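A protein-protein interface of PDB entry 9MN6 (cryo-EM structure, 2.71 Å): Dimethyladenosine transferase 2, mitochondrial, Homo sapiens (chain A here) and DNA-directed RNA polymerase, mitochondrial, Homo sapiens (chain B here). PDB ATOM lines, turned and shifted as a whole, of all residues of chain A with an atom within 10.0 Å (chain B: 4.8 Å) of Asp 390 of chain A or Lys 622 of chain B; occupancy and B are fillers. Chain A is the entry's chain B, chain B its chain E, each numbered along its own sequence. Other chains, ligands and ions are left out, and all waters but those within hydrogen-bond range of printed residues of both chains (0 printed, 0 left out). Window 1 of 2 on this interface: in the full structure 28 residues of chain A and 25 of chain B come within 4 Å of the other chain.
Printed residues of chain A that touch a printed residue of chain B: Arg 340, Ser 341, Pro 344, Leu 388, Asp 390, Glu 391, Thr 392, Leu 393, Asp 395 and Arg 396. Hydrophobic or aromatic side chains of chain A within 4 Å of the printed part of chain B: Pro 344, Leu 388 and Leu 393. Among the printed residues, 18 pairs touch across the chains. Among the printed residues, Asp or Glu carboxylates within 4 Å of a Lys or Arg side-chain nitrogen of the other chain: Asp 390 of chain A with Arg 770 of chain B (3.4 Å) and Glu 391 of chain A with Arg 770 of chain B (3.7 Å).
Asp 390 of chain A touches just these residues of chain B: Lys 622 and Arg 770. Lys 622 of chain B touches two residues of chain A. No residue of chain A comes within 4 Å of Leu 621 of chain B. No residue of chain A comes within 4 Å of Pro 623 of chain B. Of the printed residues of chain B, Pro 344 of chain A touches Tyr 607 and His 624. Printed residues of chain B within 4 Å of Arg 340 of chain A: Tyr 607. Of the printed residues of chain B, Glu 391 of chain A touches Arg 770.
Among the printed residues, merely in contact across the chains: Arg 340 of chain A with Tyr 607 of chain B (3.1 Å), Ser 341 of chain A with Tyr 607 of chain B (3.8 Å), Ser 341 of chain A with Val 609 of chain B (3.3 Å), Pro 344 of chain A with Tyr 607 of chain B (3.5 Å), Pro 344 of chain A with His 624 of chain B (3.4 Å), Leu 388 of chain A with Tyr 607 of chain B (3.6 Å), Leu 388 of chain A with His 624 of chain B (3.9 Å), Asp 390 of chain A with Lys 622 of chain B (3.7 Å), Thr 392 of chain A with Gln 493 of chain B (3.7 Å), Leu 393 of chain A with Val 609 of chain B (3.7 Å), Asp 395 of chain A with Gln 493 of chain B (3.6 Å) and Arg 396 of chain A with Ile 620 of chain B (3.7 Å).
The backbone carbonyl oxygen of Val 609 of chain B is in hydrogen-bond range of the backbone NH of Ile 620 of chain B, at 2.9 Å. N of His 624 of chain B sits at hydrogen-bond distance from O of Val 605 of chain B, 3.0 Å away. O of Tyr 607 of chain B is in hydrogen-bond range of N of Lys 622 of chain B, at 2.9 Å.
The side-chain amino group (NZ) of Lys 622 of chain B is in hydrogen-bond range of the backbone carbonyl oxygen (O) of Leu 388 of chain A (2.4 Å). The guanidinium group of Arg 770 of chain B lies within salt-bridge range of the side-chain carboxylate of Glu 391 of chain A. NH2 of Arg 396 of chain A lies within hydrogen-bond range of O of Gly 494 of chain B, at 3.4 Å. N of Thr 392 of chain A sits close to NH1 of Arg 770 of chain B, at 3.4 Å. NH1 of Arg 770 of chain B lies within salt-bridge range of OD1 of Asp 390 of chain A. The backbone carbonyl oxygen (O) of Arg 396 of chain A sits close to the backbone carbonyl oxygen (O) of Gln 493 of chain B (2.9 Å).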
ATOM      1  N   ASN A 318     -31.303   6.342  15.740  1.00  0.00           N
ATOM      2  CA  ASN A 318     -30.300   5.320  16.034  1.00  0.00           C
ATOM      3  C   ASN A 318     -29.573   5.606  17.340  1.00  0.00           C
ATOM      4  O   ASN A 318     -29.163   4.670  18.035  1.00  0.00           O
ATOM      5  CB  ASN A 318     -29.282   5.212  14.899  1.00  0.00           C
ATOM      6  CG  ASN A 318     -29.923   4.924  13.565  1.00  0.00           C
ATOM      7  OD1 ASN A 318     -30.563   5.789  12.975  1.00  0.00           O
ATOM      8  ND2 ASN A 318     -29.755   3.701  13.079  1.00  0.00           N
ATOM      9  N   ILE A 319     -29.403   6.884  17.678  1.00  0.00           N
ATOM     10  CA  ILE A 319     -28.795   7.262  18.951  1.00  0.00           C
ATOM     11  C   ILE A 319     -29.664   6.790  20.111  1.00  0.00           C
ATOM     12  O   ILE A 319     -29.166   6.250  21.107  1.00  0.00           O
ATOM     13  CB  ILE A 319     -28.574   8.784  18.984  1.00  0.00           C
ATOM     14  CG1 ILE A 319     -27.598   9.205  17.887  1.00  0.00           C
ATOM     15  CG2 ILE A 319     -28.003   9.204  20.306  1.00  0.00           C
ATOM     16  CD1 ILE A 319     -27.521  10.701  17.681  1.00  0.00           C
ATOM     17  N   PHE A 320     -30.981   6.966  19.983  1.00  0.00           N
ATOM     18  CA  PHE A 320     -31.926   6.508  20.999  1.00  0.00           C
ATOM     19  C   PHE A 320     -31.953   4.984  21.078  1.00  0.00           C
ATOM     20  O   PHE A 320     -32.043   4.410  22.174  1.00  0.00           O
ATOM     21  CB  PHE A 320     -33.305   7.082  20.672  1.00  0.00           C
ATOM     22  CG  PHE A 320     -34.401   6.621  21.579  1.00  0.00           C
ATOM     23  CD1 PHE A 320     -34.483   7.098  22.875  1.00  0.00           C
ATOM     24  CD2 PHE A 320     -35.379   5.751  21.125  1.00  0.00           C
ATOM     25  CE1 PHE A 320     -35.500   6.701  23.709  1.00  0.00           C
ATOM     26  CE2 PHE A 320     -36.400   5.346  21.957  1.00  0.00           C
ATOM     27  CZ  PHE A 320     -36.460   5.824  23.250  1.00  0.00           C
ATOM     28  N   HIS A 322     -29.416   3.031  20.397  1.00  0.00           N
ATOM     29  CA  HIS A 322     -28.181   2.656  21.072  1.00  0.00           C
ATOM     30  C   HIS A 322     -28.253   2.930  22.567  1.00  0.00           C
ATOM     31  O   HIS A 322     -27.680   2.171  23.357  1.00  0.00           O
ATOM     32  CB  HIS A 322     -26.992   3.395  20.470  1.00  0.00           C
ATOM     33  CG  HIS A 322     -25.673   2.811  20.864  1.00  0.00           C
ATOM     34  ND1 HIS A 322     -25.292   1.536  20.511  1.00  0.00           N
ATOM     35  CD2 HIS A 322     -24.656   3.319  21.600  1.00  0.00           C
ATOM     36  CE1 HIS A 322     -24.090   1.290  20.995  1.00  0.00           C
ATOM     37  NE2 HIS A 322     -23.682   2.354  21.662  1.00  0.00           N
ATOM     38  N   LEU A 323     -28.924   4.019  22.967  1.00  0.00           N
ATOM     39  CA  LEU A 323     -29.188   4.253  24.387  1.00  0.00           C
ATOM     40  C   LEU A 323     -29.934   3.082  24.999  1.00  0.00           C
ATOM     41  O   LEU A 323     -29.559   2.592  26.070  1.00  0.00           O
ATOM     42  CB  LEU A 323     -29.990   5.546  24.590  1.00  0.00           C
ATOM     43  CG  LEU A 323     -30.260   6.084  26.012  1.00  0.00           C
ATOM     44  CD1 LEU A 323     -30.424   7.568  25.973  1.00  0.00           C
ATOM     45  CD2 LEU A 323     -31.519   5.519  26.679  1.00  0.00           C
ATOM     46  N   ARG A 340     -22.759   7.220  32.382  1.00  0.00           N
ATOM     47  CA  ARG A 340     -21.353   7.612  32.454  1.00  0.00           C
ATOM     48  C   ARG A 340     -20.580   7.107  31.246  1.00  0.00           C
ATOM     49  O   ARG A 340     -19.567   7.703  30.866  1.00  0.00           O
ATOM     50  CB  ARG A 340     -20.688   7.112  33.737  1.00  0.00           C
ATOM     51  CG  ARG A 340     -21.075   7.857  35.002  1.00  0.00           C
ATOM     52  CD  ARG A 340     -20.890   6.982  36.228  1.00  0.00           C
ATOM     53  NE  ARG A 340     -20.911   7.764  37.458  1.00  0.00           N
ATOM     54  CZ  ARG A 340     -20.780   7.252  38.674  1.00  0.00           C
ATOM     55  NH1 ARG A 340     -20.617   5.953  38.864  1.00  0.00           N
ATOM     56  NH2 ARG A 340     -20.813   8.064  39.726  1.00  0.00           N
ATOM     57  N   SER A 341     -21.031   6.009  30.640  1.00  0.00           N
ATOM     58  CA  SER A 341     -20.416   5.519  29.415  1.00  0.00           C
ATOM     59  C   SER A 341     -21.068   6.088  28.161  1.00  0.00           C
ATOM     60  O   SER A 341     -20.463   6.024  27.086  1.00  0.00           O
ATOM     61  CB  SER A 341     -20.474   3.993  29.377  1.00  0.00           C
ATOM     62  OG  SER A 341     -19.771   3.428  30.470  1.00  0.00           O
ATOM     63  N   LEU A 342     -22.275   6.643  28.271  1.00  0.00           N
ATOM     64  CA  LEU A 342     -22.993   7.125  27.097  1.00  0.00           C
ATOM     65  C   LEU A 342     -22.780   8.604  26.803  1.00  0.00           C
ATOM     66  O   LEU A 342     -22.797   8.990  25.629  1.00  0.00           O
ATOM     67  CB  LEU A 342     -24.494   6.870  27.250  1.00  0.00           C
ATOM     68  CG  LEU A 342     -25.011   5.513  26.775  1.00  0.00           C
ATOM     69  CD1 LEU A 342     -26.528   5.504  26.749  1.00  0.00           C
ATOM     70  CD2 LEU A 342     -24.440   5.147  25.412  1.00  0.00           C
ATOM     71  N   PRO A 344     -20.835  12.567  28.200  1.00  0.00           N
ATOM     72  CA  PRO A 344     -20.030  13.310  29.180  1.00  0.00           C
ATOM     73  C   PRO A 344     -20.860  14.091  30.179  1.00  0.00           C
ATOM     74  O   PRO A 344     -20.302  14.574  31.173  1.00  0.00           O
ATOM     75  CB  PRO A 344     -19.205  14.258  28.305  1.00  0.00           C
ATOM     76  CG  PRO A 344     -20.060  14.451  27.100  1.00  0.00           C
ATOM     77  CD  PRO A 344     -20.644  13.098  26.840  1.00  0.00           C
ATOM     78  N   TYR A 385     -20.492  18.480  22.537  1.00  0.00           N
ATOM     79  CA  TYR A 385     -20.479  17.032  22.371  1.00  0.00           C
ATOM     80  C   TYR A 385     -21.419  16.422  23.401  1.00  0.00           C
ATOM     81  O   TYR A 385     -21.089  16.348  24.589  1.00  0.00           O
ATOM     82  CB  TYR A 385     -19.063  16.484  22.517  1.00  0.00           C
ATOM     83  CG  TYR A 385     -18.154  16.841  21.367  1.00  0.00           C
ATOM     84  CD1 TYR A 385     -18.426  16.397  20.079  1.00  0.00           C
ATOM     85  CD2 TYR A 385     -17.023  17.625  21.566  1.00  0.00           C
ATOM     86  CE1 TYR A 385     -17.598  16.722  19.021  1.00  0.00           C
ATOM     87  CE2 TYR A 385     -16.188  17.957  20.514  1.00  0.00           C
ATOM     88  CZ  TYR A 385     -16.480  17.502  19.244  1.00  0.00           C
ATOM     89  OH  TYR A 385     -15.654  17.827  18.194  1.00  0.00           O
ATOM     90  N   LYS A 386     -22.594  15.989  22.950  1.00  0.00           N
ATOM     91  CA  LYS A 386     -23.612  15.455  23.844  1.00  0.00           C
ATOM     92  C   LYS A 386     -23.656  13.937  23.869  1.00  0.00           C
ATOM     93  O   LYS A 386     -24.055  13.360  24.884  1.00  0.00           O
ATOM     94  CB  LYS A 386     -24.992  15.991  23.454  1.00  0.00           C
ATOM     95  CG  LYS A 386     -25.222  17.440  23.847  1.00  0.00           C
ATOM     96  CD  LYS A 386     -26.544  17.967  23.313  1.00  0.00           C
ATOM     97  CE  LYS A 386     -26.641  17.815  21.806  1.00  0.00           C
ATOM     98  NZ  LYS A 386     -27.840  18.509  21.263  1.00  0.00           N
ATOM     99  N   TRP A 387     -23.259  13.276  22.787  1.00  0.00           N
ATOM    100  CA  TRP A 387     -23.297  11.826  22.719  1.00  0.00           C
ATOM    101  C   TRP A 387     -21.981  11.315  22.158  1.00  0.00           C
ATOM    102  O   TRP A 387     -21.262  12.039  21.465  1.00  0.00           O
ATOM    103  CB  TRP A 387     -24.431  11.313  21.833  1.00  0.00           C
ATOM    104  CG  TRP A 387     -25.782  11.804  22.208  1.00  0.00           C
ATOM    105  CD1 TRP A 387     -26.315  13.031  21.933  1.00  0.00           C
ATOM    106  CD2 TRP A 387     -26.758  11.108  22.982  1.00  0.00           C
ATOM    107  NE1 TRP A 387     -27.580  13.125  22.454  1.00  0.00           N
ATOM    108  CE2 TRP A 387     -27.875  11.959  23.108  1.00  0.00           C
ATOM    109  CE3 TRP A 387     -26.803   9.843  23.573  1.00  0.00           C
ATOM    110  CZ2 TRP A 387     -29.022  11.581  23.791  1.00  0.00           C
ATOM    111  CZ3 TRP A 387     -27.939   9.473  24.249  1.00  0.00           C
ATOM    112  CH2 TRP A 387     -29.031  10.343  24.361  1.00  0.00           C
ATOM    113  N   LEU A 388     -21.671  10.057  22.460  1.00  0.00           N
ATOM    114  CA  LEU A 388     -20.528   9.415  21.833  1.00  0.00           C
ATOM    115  C   LEU A 388     -20.910   8.413  20.758  1.00  0.00           C
ATOM    116  O   LEU A 388     -20.014   7.803  20.163  1.00  0.00           O
ATOM    117  CB  LEU A 388     -19.648   8.706  22.865  1.00  0.00           C
ATOM    118  CG  LEU A 388     -18.660   9.564  23.657  1.00  0.00           C
ATOM    119  CD1 LEU A 388     -19.310  10.350  24.786  1.00  0.00           C
ATOM    120  CD2 LEU A 388     -17.520   8.710  24.147  1.00  0.00           C
ATOM    121  N   TYR A 389     -22.198   8.214  20.496  1.00  0.00           N
ATOM    122  CA  TYR A 389     -22.574   7.254  19.472  1.00  0.00           C
ATOM    123  C   TYR A 389     -22.340   7.837  18.085  1.00  0.00           C
ATOM    124  O   TYR A 389     -22.601   9.015  17.828  1.00  0.00           O
ATOM    125  CB  TYR A 389     -24.032   6.816  19.631  1.00  0.00           C
ATOM    126  CG  TYR A 389     -24.537   5.957  18.486  1.00  0.00           C
ATOM    127  CD1 TYR A 389     -24.253   4.600  18.446  1.00  0.00           C
ATOM    128  CD2 TYR A 389     -25.325   6.488  17.471  1.00  0.00           C
ATOM    129  CE1 TYR A 389     -24.712   3.799  17.420  1.00  0.00           C
ATOM    130  CE2 TYR A 389     -25.789   5.692  16.436  1.00  0.00           C
ATOM    131  CZ  TYR A 389     -25.478   4.347  16.420  1.00  0.00           C
ATOM    132  OH  TYR A 389     -25.934   3.546  15.402  1.00  0.00           O
ATOM    133  N   ASP A 390     -21.839   6.989  17.196  1.00  0.00           N
ATOM    134  CA  ASP A 390     -21.575   7.333  15.811  1.00  0.00           C
ATOM    135  C   ASP A 390     -21.623   6.004  15.067  1.00  0.00           C
ATOM    136  O   ASP A 390     -21.566   4.939  15.686  1.00  0.00           O
ATOM    137  CB  ASP A 390     -20.236   8.092  15.709  1.00  0.00           C
ATOM    138  CG  ASP A 390     -19.791   8.354  14.285  1.00  0.00           C
ATOM    139  OD1 ASP A 390     -20.656   8.579  13.419  1.00  0.00           O
ATOM    140  OD2 ASP A 390     -18.568   8.373  14.042  1.00  0.00           O
ATOM    141  N   GLU A 391     -21.760   6.054  13.735  1.00  0.00           N
ATOM    142  CA  GLU A 391     -21.870   4.813  12.968  1.00  0.00           C
ATOM    143  C   GLU A 391     -20.593   3.974  13.002  1.00  0.00           C
ATOM    144  O   GLU A 391     -20.641   2.783  12.667  1.00  0.00           O
ATOM    145  CB  GLU A 391     -22.278   5.090  11.514  1.00  0.00           C
ATOM    146  CG  GLU A 391     -23.703   5.629  11.304  1.00  0.00           C
ATOM    147  CD  GLU A 391     -23.874   7.098  11.644  1.00  0.00           C
ATOM    148  OE1 GLU A 391     -22.861   7.784  11.873  1.00  0.00           O
ATOM    149  OE2 GLU A 391     -25.032   7.568  11.677  1.00  0.00           O
ATOM    150  N   THR A 392     -19.468   4.549  13.448  1.00  0.00           N
ATOM    151  CA  THR A 392     -18.259   3.764  13.692  1.00  0.00           C
ATOM    152  C   THR A 392     -18.452   2.729  14.794  1.00  0.00           C
ATOM    153  O   THR A 392     -17.653   1.795  14.907  1.00  0.00           O
ATOM    154  CB  THR A 392     -17.092   4.677  14.062  1.00  0.00           C
ATOM    155  OG1 THR A 392     -17.329   5.262  15.349  1.00  0.00           O
ATOM    156  CG2 THR A 392     -16.912   5.762  13.035  1.00  0.00           C
ATOM    157  N   LEU A 393     -19.487   2.878  15.623  1.00  0.00           N
ATOM    158  CA  LEU A 393     -19.793   1.856  16.613  1.00  0.00           C
ATOM    159  C   LEU A 393     -20.533   0.663  16.023  1.00  0.00           C
ATOM    160  O   LEU A 393     -20.904  -0.240  16.782  1.00  0.00           O
ATOM    161  CB  LEU A 393     -20.606   2.451  17.761  1.00  0.00           C
ATOM    162  CG  LEU A 393     -19.835   3.440  18.635  1.00  0.00           C
ATOM    163  CD1 LEU A 393     -20.735   4.031  19.706  1.00  0.00           C
ATOM    164  CD2 LEU A 393     -18.605   2.791  19.239  1.00  0.00           C
ATOM    165  N   GLU A 394     -20.783   0.647  14.709  1.00  0.00           N
ATOM    166  CA  GLU A 394     -21.296  -0.564  14.076  1.00  0.00           C
ATOM    167  C   GLU A 394     -20.283  -1.701  14.180  1.00  0.00           C
ATOM    168  O   GLU A 394     -20.645  -2.851  14.453  1.00  0.00           O
ATOM    169  CB  GLU A 394     -21.659  -0.285  12.616  1.00  0.00           C
ATOM    170  CG  GLU A 394     -22.973   0.470  12.425  1.00  0.00           C
ATOM    171  CD  GLU A 394     -24.206  -0.364  12.741  1.00  0.00           C
ATOM    172  OE1 GLU A 394     -24.098  -1.606  12.824  1.00  0.00           O
ATOM    173  OE2 GLU A 394     -25.293   0.228  12.911  1.00  0.00           O
ATOM    174  N   ASP A 395     -19.006  -1.393  13.962  1.00  0.00           N
ATOM    175  CA  ASP A 395     -17.913  -2.323  14.215  1.00  0.00           C
ATOM    176  C   ASP A 395     -16.720  -1.543  14.752  1.00  0.00           C
ATOM    177  O   ASP A 395     -16.281  -0.571  14.127  1.00  0.00           O
ATOM    178  CB  ASP A 395     -17.538  -3.106  12.948  1.00  0.00           C
ATOM    179  CG  ASP A 395     -17.245  -2.206  11.765  1.00  0.00           C
ATOM    180  OD1 ASP A 395     -18.136  -1.422  11.376  1.00  0.00           O
ATOM    181  OD2 ASP A 395     -16.117  -2.275  11.233  1.00  0.00           O
ATOM    182  N   ARG A 396     -16.207  -1.980  15.905  1.00  0.00           N
ATOM    183  CA  ARG A 396     -15.150  -1.294  16.662  1.00  0.00           C
ATOM    184  C   ARG A 396     -15.486   0.169  16.947  1.00  0.00           C
ATOM    185  O   ARG A 396     -14.707   1.067  16.630  1.00  0.00           O
ATOM    186  CB  ARG A 396     -13.800  -1.384  15.939  1.00  0.00           C
ATOM    187  CG  ARG A 396     -13.227  -2.785  15.846  1.00  0.00           C
ATOM    188  CD  ARG A 396     -12.132  -2.854  14.781  1.00  0.00           C
ATOM    189  NE  ARG A 396     -11.097  -1.837  14.945  1.00  0.00           N
ATOM    190  CZ  ARG A 396     -10.210  -1.788  15.933  1.00  0.00           C
ATOM    191  NH1 ARG A 396     -10.131  -2.742  16.849  1.00  0.00           N
ATOM    192  NH2 ARG A 396      -9.362  -0.765  15.992  1.00  0.00           N
ATOM    193  N   ALA B 492     -10.115   7.100  16.550  1.00  0.00           N
ATOM    194  CA  ALA B 492     -11.320   7.782  17.015  1.00  0.00           C
ATOM    195  C   ALA B 492     -12.500   6.828  17.142  1.00  0.00           C
ATOM    196  O   ALA B 492     -13.376   7.039  17.988  1.00  0.00           O
ATOM    197  CB  ALA B 492     -11.669   8.933  16.074  1.00  0.00           C
ATOM    198  N   GLN B 493     -12.544   5.778  16.317  1.00  0.00           N
ATOM    199  CA  GLN B 493     -13.612   4.793  16.435  1.00  0.00           C
ATOM    200  C   GLN B 493     -13.454   3.938  17.684  1.00  0.00           C
ATOM    201  O   GLN B 493     -14.453   3.487  18.256  1.00  0.00           O
ATOM    202  CB  GLN B 493     -13.660   3.909  15.189  1.00  0.00           C
ATOM    203  CG  GLN B 493     -12.352   3.233  14.830  1.00  0.00           C
ATOM    204  CD  GLN B 493     -12.535   2.124  13.820  1.00  0.00           C
ATOM    205  OE1 GLN B 493     -13.652   1.847  13.382  1.00  0.00           O
ATOM    206  NE2 GLN B 493     -11.439   1.478  13.444  1.00  0.00           N
ATOM    207  N   GLY B 494     -12.222   3.709  18.126  1.00  0.00           N
ATOM    208  CA  GLY B 494     -11.952   2.903  19.296  1.00  0.00           C
ATOM    209  C   GLY B 494     -11.518   1.492  18.938  1.00  0.00           C
ATOM    210  O   GLY B 494     -11.628   1.033  17.797  1.00  0.00           O
ATOM    211  N   VAL B 605     -11.163  10.245  29.851  1.00  0.00           N
ATOM    212  CA  VAL B 605     -10.587  10.394  28.520  1.00  0.00           C
ATOM    213  C   VAL B 605     -11.139   9.326  27.585  1.00  0.00           C
ATOM    214  O   VAL B 605     -11.533   9.617  26.449  1.00  0.00           O
ATOM    215  CB  VAL B 605      -9.050  10.345  28.598  1.00  0.00           C
ATOM    216  CG1 VAL B 605      -8.433  10.270  27.210  1.00  0.00           C
ATOM    217  CG2 VAL B 605      -8.523  11.546  29.358  1.00  0.00           C
ATOM    218  N   LEU B 606     -11.203   8.085  28.054  1.00  0.00           N
ATOM    219  CA  LEU B 606     -11.707   6.972  27.267  1.00  0.00           C
ATOM    220  C   LEU B 606     -13.035   6.512  27.841  1.00  0.00           C
ATOM    221  O   LEU B 606     -13.238   6.526  29.059  1.00  0.00           O
ATOM    222  CB  LEU B 606     -10.725   5.800  27.260  1.00  0.00           C
ATOM    223  CG  LEU B 606      -9.316   6.089  26.746  1.00  0.00           C
ATOM    224  CD1 LEU B 606      -8.493   4.807  26.707  1.00  0.00           C
ATOM    225  CD2 LEU B 606      -9.348   6.784  25.397  1.00  0.00           C
ATOM    226  N   TYR B 607     -13.943   6.096  26.962  1.00  0.00           N
ATOM    227  CA  TYR B 607     -15.255   5.634  27.376  1.00  0.00           C
ATOM    228  C   TYR B 607     -15.444   4.200  26.916  1.00  0.00           C
ATOM    229  O   TYR B 607     -15.062   3.839  25.798  1.00  0.00           O
ATOM    230  CB  TYR B 607     -16.366   6.506  26.798  1.00  0.00           C
ATOM    231  CG  TYR B 607     -16.516   7.856  27.458  1.00  0.00           C
ATOM    232  CD1 TYR B 607     -15.648   8.896  27.160  1.00  0.00           C
ATOM    233  CD2 TYR B 607     -17.536   8.097  28.364  1.00  0.00           C
ATOM    234  CE1 TYR B 607     -15.788  10.131  27.749  1.00  0.00           C
ATOM    235  CE2 TYR B 607     -17.679   9.331  28.961  1.00  0.00           C
ATOM    236  CZ  TYR B 607     -16.802  10.341  28.652  1.00  0.00           C
ATOM    237  OH  TYR B 607     -16.946  11.571  29.245  1.00  0.00           O
ATOM    238  N   VAL B 609     -17.855   1.799  25.668  1.00  0.00           N
ATOM    239  CA  VAL B 609     -19.158   1.690  25.031  1.00  0.00           C
ATOM    240  C   VAL B 609     -19.320   0.278  24.480  1.00  0.00           C
ATOM    241  O   VAL B 609     -18.382  -0.303  23.923  1.00  0.00           O
ATOM    242  CB  VAL B 609     -19.345   2.764  23.945  1.00  0.00           C
ATOM    243  CG1 VAL B 609     -19.355   4.141  24.579  1.00  0.00           C
ATOM    244  CG2 VAL B 609     -18.227   2.710  22.918  1.00  0.00           C
ATOM    245  N   ILE B 620     -15.863  -1.651  23.498  1.00  0.00           N
ATOM    246  CA  ILE B 620     -14.993  -0.807  22.692  1.00  0.00           C
ATOM    247  C   ILE B 620     -14.624   0.415  23.516  1.00  0.00           C
ATOM    248  O   ILE B 620     -15.502   1.081  24.078  1.00  0.00           O
ATOM    249  CB  ILE B 620     -15.673  -0.392  21.373  1.00  0.00           C
ATOM    250  CG1 ILE B 620     -16.076  -1.626  20.568  1.00  0.00           C
ATOM    251  CG2 ILE B 620     -14.762   0.507  20.551  1.00  0.00           C
ATOM    252  CD1 ILE B 620     -14.931  -2.521  20.207  1.00  0.00           C
ATOM    253  N   LEU B 621     -13.330   0.709  23.590  1.00  0.00           N
ATOM    254  CA  LEU B 621     -12.861   1.903  24.288  1.00  0.00           C
ATOM    255  C   LEU B 621     -12.734   3.013  23.260  1.00  0.00           C
ATOM    256  O   LEU B 621     -11.736   3.105  22.543  1.00  0.00           O
ATOM    257  CB  LEU B 621     -11.542   1.668  25.014  1.00  0.00           C
ATOM    258  CG  LEU B 621     -11.608   1.043  26.409  1.00  0.00           C
ATOM    259  CD1 LEU B 621     -12.377   1.977  27.331  1.00  0.00           C
ATOM    260  CD2 LEU B 621     -12.180  -0.354  26.430  1.00  0.00           C
ATOM    261  N   LYS B 622     -13.742   3.863  23.199  1.00  0.00           N
ATOM    262  CA  LYS B 622     -13.724   4.963  22.264  1.00  0.00           C
ATOM    263  C   LYS B 622     -13.249   6.217  22.974  1.00  0.00           C
ATOM    264  O   LYS B 622     -13.714   6.506  24.084  1.00  0.00           O
ATOM    265  CB  LYS B 622     -15.119   5.184  21.665  1.00  0.00           C
ATOM    266  CG  LYS B 622     -15.239   6.412  20.782  1.00  0.00           C
ATOM    267  CD  LYS B 622     -16.632   6.527  20.189  1.00  0.00           C
ATOM    268  CE  LYS B 622     -16.764   7.780  19.345  1.00  0.00           C
ATOM    269  NZ  LYS B 622     -18.095   7.863  18.687  1.00  0.00           N
ATOM    270  N   PRO B 623     -12.293   6.946  22.406  1.00  0.00           N
ATOM    271  CA  PRO B 623     -11.882   8.213  23.012  1.00  0.00           C
ATOM    272  C   PRO B 623     -12.995   9.241  22.922  1.00  0.00           C
ATOM    273  O   PRO B 623     -13.858   9.182  22.043  1.00  0.00           O
ATOM    274  CB  PRO B 623     -10.665   8.627  22.180  1.00  0.00           C
ATOM    275  CG  PRO B 623     -10.874   7.961  20.866  1.00  0.00           C
ATOM    276  CD  PRO B 623     -11.546   6.654  21.171  1.00  0.00           C
ATOM    277  N   HIS B 624     -12.978  10.173  23.866  1.00  0.00           N
ATOM    278  CA  HIS B 624     -13.999  11.206  23.897  1.00  0.00           C
ATOM    279  C   HIS B 624     -13.819  12.130  22.694  1.00  0.00           C
ATOM    280  O   HIS B 624     -12.680  12.414  22.301  1.00  0.00           O
ATOM    281  CB  HIS B 624     -13.912  12.000  25.200  1.00  0.00           C
ATOM    282  CG  HIS B 624     -14.976  13.040  25.343  1.00  0.00           C
ATOM    283  ND1 HIS B 624     -16.301  12.720  25.548  1.00  0.00           N
ATOM    284  CD2 HIS B 624     -14.922  14.390  25.280  1.00  0.00           C
ATOM    285  CE1 HIS B 624     -17.012  13.831  25.620  1.00  0.00           C
ATOM    286  NE2 HIS B 624     -16.198  14.859  25.466  1.00  0.00           N
ATOM    287  N   ARG B 770     -15.161   8.572   5.906  1.00  0.00           N
ATOM    288  CA  ARG B 770     -14.468   7.716   6.864  1.00  0.00           C
ATOM    289  C   ARG B 770     -13.616   6.655   6.173  1.00  0.00           C
ATOM    290  O   ARG B 770     -12.548   6.290   6.689  1.00  0.00           O
ATOM    291  CB  ARG B 770     -15.483   7.082   7.808  1.00  0.00           C
ATOM    292  CG  ARG B 770     -15.737   7.943   9.026  1.00  0.00           C
ATOM    293  CD  ARG B 770     -16.915   7.454   9.824  1.00  0.00           C
ATOM    294  NE  ARG B 770     -18.162   7.492   9.070  1.00  0.00           N
ATOM    295  CZ  ARG B 770     -19.338   7.145   9.571  1.00  0.00           C
ATOM    296  NH1 ARG B 770     -19.463   6.744  10.826  1.00  0.00           N
ATOM    297  NH2 ARG B 770     -20.417   7.202   8.795  1.00  0.00           N
